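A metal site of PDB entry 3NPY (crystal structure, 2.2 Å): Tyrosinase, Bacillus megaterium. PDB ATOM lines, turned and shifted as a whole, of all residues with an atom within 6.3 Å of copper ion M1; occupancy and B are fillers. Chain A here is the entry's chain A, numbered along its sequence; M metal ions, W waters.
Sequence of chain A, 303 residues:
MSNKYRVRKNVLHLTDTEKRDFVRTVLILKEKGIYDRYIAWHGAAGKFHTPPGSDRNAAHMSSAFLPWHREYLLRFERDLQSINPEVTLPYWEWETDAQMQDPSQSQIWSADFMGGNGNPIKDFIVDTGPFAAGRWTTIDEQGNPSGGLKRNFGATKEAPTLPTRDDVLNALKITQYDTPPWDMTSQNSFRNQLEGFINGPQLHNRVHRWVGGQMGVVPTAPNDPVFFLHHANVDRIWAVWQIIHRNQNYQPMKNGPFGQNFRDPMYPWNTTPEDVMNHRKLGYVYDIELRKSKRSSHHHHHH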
ATOM      1  N   HIS A  42     -32.123  -1.445 -20.602  1.00  0.00           N
ATOM      2  CA  HIS A  42     -30.812  -1.064 -21.101  1.00  0.00           C
ATOM      3  C   HIS A  42     -29.737  -1.991 -20.556  1.00  0.00           C
ATOM      4  O   HIS A  42     -28.809  -2.370 -21.265  1.00  0.00           O
ATOM      5  CB  HIS A  42     -30.562   0.392 -20.740  1.00  0.00           C
ATOM      6  CG  HIS A  42     -29.170   0.867 -21.041  1.00  0.00           C
ATOM      7  ND1 HIS A  42     -28.148   0.802 -20.117  1.00  0.00           N
ATOM      8  CD2 HIS A  42     -28.640   1.447 -22.141  1.00  0.00           C
ATOM      9  CE1 HIS A  42     -27.052   1.327 -20.639  1.00  0.00           C
ATOM     10  NE2 HIS A  42     -27.333   1.729 -21.866  1.00  0.00           N
ATOM     11  N   HIS A  60     -25.387  -1.834 -27.971  1.00  0.00           N
ATOM     12  CA  HIS A  60     -24.108  -1.175 -28.215  1.00  0.00           C
ATOM     13  C   HIS A  60     -23.161  -2.075 -29.008  1.00  0.00           C
ATOM     14  O   HIS A  60     -23.475  -3.234 -29.269  1.00  0.00           O
ATOM     15  CB  HIS A  60     -23.459  -0.753 -26.900  1.00  0.00           C
ATOM     16  CG  HIS A  60     -24.430  -0.318 -25.854  1.00  0.00           C
ATOM     17  ND1 HIS A  60     -25.279  -1.198 -25.224  1.00  0.00           N
ATOM     18  CD2 HIS A  60     -24.694   0.900 -25.329  1.00  0.00           C
ATOM     19  CE1 HIS A  60     -26.026  -0.541 -24.349  1.00  0.00           C
ATOM     20  NE2 HIS A  60     -25.688   0.739 -24.399  1.00  0.00           N
ATOM     21  N   PHE A  65     -26.985   0.035 -32.325  1.00  0.00           N
ATOM     22  CA  PHE A  65     -26.814   1.093 -31.344  1.00  0.00           C
ATOM     23  C   PHE A  65     -27.772   2.280 -31.519  1.00  0.00           C
ATOM     24  O   PHE A  65     -28.460   2.690 -30.586  1.00  0.00           O
ATOM     25  CB  PHE A  65     -25.373   1.597 -31.360  1.00  0.00           C
ATOM     26  CG  PHE A  65     -25.156   2.851 -30.547  1.00  0.00           C
ATOM     27  CD1 PHE A  65     -25.310   2.818 -29.165  1.00  0.00           C
ATOM     28  CD2 PHE A  65     -24.801   4.041 -31.167  1.00  0.00           C
ATOM     29  CE1 PHE A  65     -25.126   3.987 -28.405  1.00  0.00           C
ATOM     30  CE2 PHE A  65     -24.604   5.218 -30.416  1.00  0.00           C
ATOM     31  CZ  PHE A  65     -24.767   5.186 -29.035  1.00  0.00           C
ATOM     32  N   HIS A  69     -31.518   2.806 -29.357  1.00  0.00           N
ATOM     33  CA  HIS A  69     -31.720   3.948 -28.474  1.00  0.00           C
ATOM     34  C   HIS A  69     -32.823   4.871 -28.952  1.00  0.00           C
ATOM     35  O   HIS A  69     -33.420   5.581 -28.142  1.00  0.00           O
ATOM     36  CB  HIS A  69     -30.438   4.736 -28.286  1.00  0.00           C
ATOM     37  CG  HIS A  69     -29.462   4.069 -27.361  1.00  0.00           C
ATOM     38  ND1 HIS A  69     -28.561   3.123 -27.786  1.00  0.00           N
ATOM     39  CD2 HIS A  69     -29.285   4.185 -26.029  1.00  0.00           C
ATOM     40  CE1 HIS A  69     -27.870   2.673 -26.760  1.00  0.00           C
ATOM     41  NE2 HIS A  69     -28.285   3.304 -25.671  1.00  0.00           N
ATOM     42  N   HIS A 204     -20.444  10.226 -28.303  1.00  0.00           N
ATOM     43  CA  HIS A 204     -21.307   9.469 -27.395  1.00  0.00           C
ATOM     44  C   HIS A 204     -20.547   8.953 -26.170  1.00  0.00           C
ATOM     45  O   HIS A 204     -20.774   9.405 -25.051  1.00  0.00           O
ATOM     46  CB  HIS A 204     -21.972   8.312 -28.131  1.00  0.00           C
ATOM     47  CG  HIS A 204     -22.672   7.340 -27.225  1.00  0.00           C
ATOM     48  ND1 HIS A 204     -22.178   6.069 -26.974  1.00  0.00           N
ATOM     49  CD2 HIS A 204     -23.816   7.454 -26.514  1.00  0.00           C
ATOM     50  CE1 HIS A 204     -22.997   5.447 -26.143  1.00  0.00           C
ATOM     51  NE2 HIS A 204     -24.002   6.262 -25.857  1.00  0.00           N
ATOM     52  N   ASN A 205     -19.647   7.996 -26.395  1.00  0.00           N
ATOM     53  CA  ASN A 205     -18.918   7.355 -25.303  1.00  0.00           C
ATOM     54  C   ASN A 205     -18.239   8.396 -24.423  1.00  0.00           C
ATOM     55  O   ASN A 205     -18.109   8.207 -23.213  1.00  0.00           O
ATOM     56  CB  ASN A 205     -17.834   6.404 -25.831  1.00  0.00           C
ATOM     57  CG  ASN A 205     -18.406   5.146 -26.467  1.00  0.00           C
ATOM     58  OD1 ASN A 205     -17.685   4.411 -27.133  1.00  0.00           O
ATOM     59  ND2 ASN A 205     -19.685   4.894 -26.247  1.00  0.00           N
ATOM     60  N   HIS A 208     -20.597  10.065 -21.815  1.00  0.00           N
ATOM     61  CA  HIS A 208     -20.807   9.047 -20.781  1.00  0.00           C
ATOM     62  C   HIS A 208     -19.612   9.060 -19.801  1.00  0.00           C
ATOM     63  O   HIS A 208     -19.821   9.161 -18.626  1.00  0.00           O
ATOM     64  CB  HIS A 208     -21.067   7.626 -21.375  1.00  0.00           C
ATOM     65  CG  HIS A 208     -22.470   7.343 -21.830  1.00  0.00           C
ATOM     66  ND1 HIS A 208     -23.509   7.130 -20.964  1.00  0.00           N
ATOM     67  CD2 HIS A 208     -22.970   7.095 -23.052  1.00  0.00           C
ATOM     68  CE1 HIS A 208     -24.602   6.850 -21.641  1.00  0.00           C
ATOM     69  NE2 HIS A 208     -24.302   6.793 -22.917  1.00  0.00           N
ATOM     70  N   ALA A 221     -25.891   3.283 -16.305  1.00  0.00           N
ATOM     71  CA  ALA A 221     -26.072   4.597 -16.938  1.00  0.00           C
ATOM     72  C   ALA A 221     -27.456   5.284 -16.809  1.00  0.00           C
ATOM     73  O   ALA A 221     -27.540   6.416 -16.305  1.00  0.00           O
ATOM     74  CB  ALA A 221     -25.665   4.521 -18.405  1.00  0.00           C
ATOM     75  N   PHE A 227     -29.125  10.784 -18.954  1.00  0.00           N
ATOM     76  CA  PHE A 227     -28.908   9.752 -19.978  1.00  0.00           C
ATOM     77  C   PHE A 227     -29.837  10.005 -21.156  1.00  0.00           C
ATOM     78  O   PHE A 227     -29.429   9.885 -22.311  1.00  0.00           O
ATOM     79  CB  PHE A 227     -29.177   8.363 -19.388  1.00  0.00           C
ATOM     80  CG  PHE A 227     -29.142   7.234 -20.418  1.00  0.00           C
ATOM     81  CD1 PHE A 227     -30.218   7.013 -21.264  1.00  0.00           C
ATOM     82  CD2 PHE A 227     -28.008   6.424 -20.551  1.00  0.00           C
ATOM     83  CE1 PHE A 227     -30.188   5.997 -22.226  1.00  0.00           C
ATOM     84  CE2 PHE A 227     -27.960   5.404 -21.501  1.00  0.00           C
ATOM     85  CZ  PHE A 227     -29.043   5.195 -22.348  1.00  0.00           C
ATOM     86  N   HIS A 230     -28.874  13.166 -23.083  1.00  0.00           N
ATOM     87  CA  HIS A 230     -27.688  12.861 -23.869  1.00  0.00           C
ATOM     88  C   HIS A 230     -28.107  12.160 -25.159  1.00  0.00           C
ATOM     89  O   HIS A 230     -27.817  12.602 -26.280  1.00  0.00           O
ATOM     90  CB  HIS A 230     -26.764  11.910 -23.096  1.00  0.00           C
ATOM     91  CG  HIS A 230     -25.553  11.477 -23.869  1.00  0.00           C
ATOM     92  ND1 HIS A 230     -24.833  10.346 -23.556  1.00  0.00           N
ATOM     93  CD2 HIS A 230     -24.941  12.020 -24.950  1.00  0.00           C
ATOM     94  CE1 HIS A 230     -23.834  10.210 -24.402  1.00  0.00           C
ATOM     95  NE2 HIS A 230     -23.870  11.213 -25.260  1.00  0.00           N
ATOM     96  N   HIS A 231     -28.827  11.076 -24.997  1.00  0.00           N
ATOM     97  CA  HIS A 231     -29.221  10.276 -26.113  1.00  0.00           C
ATOM     98  C   HIS A 231     -30.108  10.998 -27.100  1.00  0.00           C
ATOM     99  O   HIS A 231     -30.045  10.741 -28.237  1.00  0.00           O
ATOM    100  CB  HIS A 231     -29.694   8.908 -25.693  1.00  0.00           C
ATOM    101  CG  HIS A 231     -28.579   7.935 -25.545  1.00  0.00           C
ATOM    102  ND1 HIS A 231     -28.064   7.254 -26.603  1.00  0.00           N
ATOM    103  CD2 HIS A 231     -27.833   7.576 -24.484  1.00  0.00           C
ATOM    104  CE1 HIS A 231     -27.089   6.479 -26.199  1.00  0.00           C
ATOM    105  NE2 HIS A 231     -26.888   6.693 -24.916  1.00  0.00           N
HETATM  106 CU    CU M   1     -25.285   5.702 -24.248  1.00  0.00          CU
HETATM  107 CU    CU M   2     -26.041   2.509 -23.235  1.00  0.00          CU
HETATM  108  O   HOH W   1     -25.596   3.925 -23.788  1.00  0.00           O
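ND2 of Asn 205 lies within hydrogen-bond range of ND1 of His 204.
Phe 227 touches copper ion M1.
The nearest printed residue that does not touch copper ion M1 is His 69 (4.1 Å).
Water W1 binds copper ion M1, at 1.9 Å.
Copper ion M1 is bound by NE2 of His 208 (2.0 Å).
Copper ion M1 is bound by NE2 of His 231.
NE2 of His 204 is bound to copper ion M1, at 2.1 Å.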
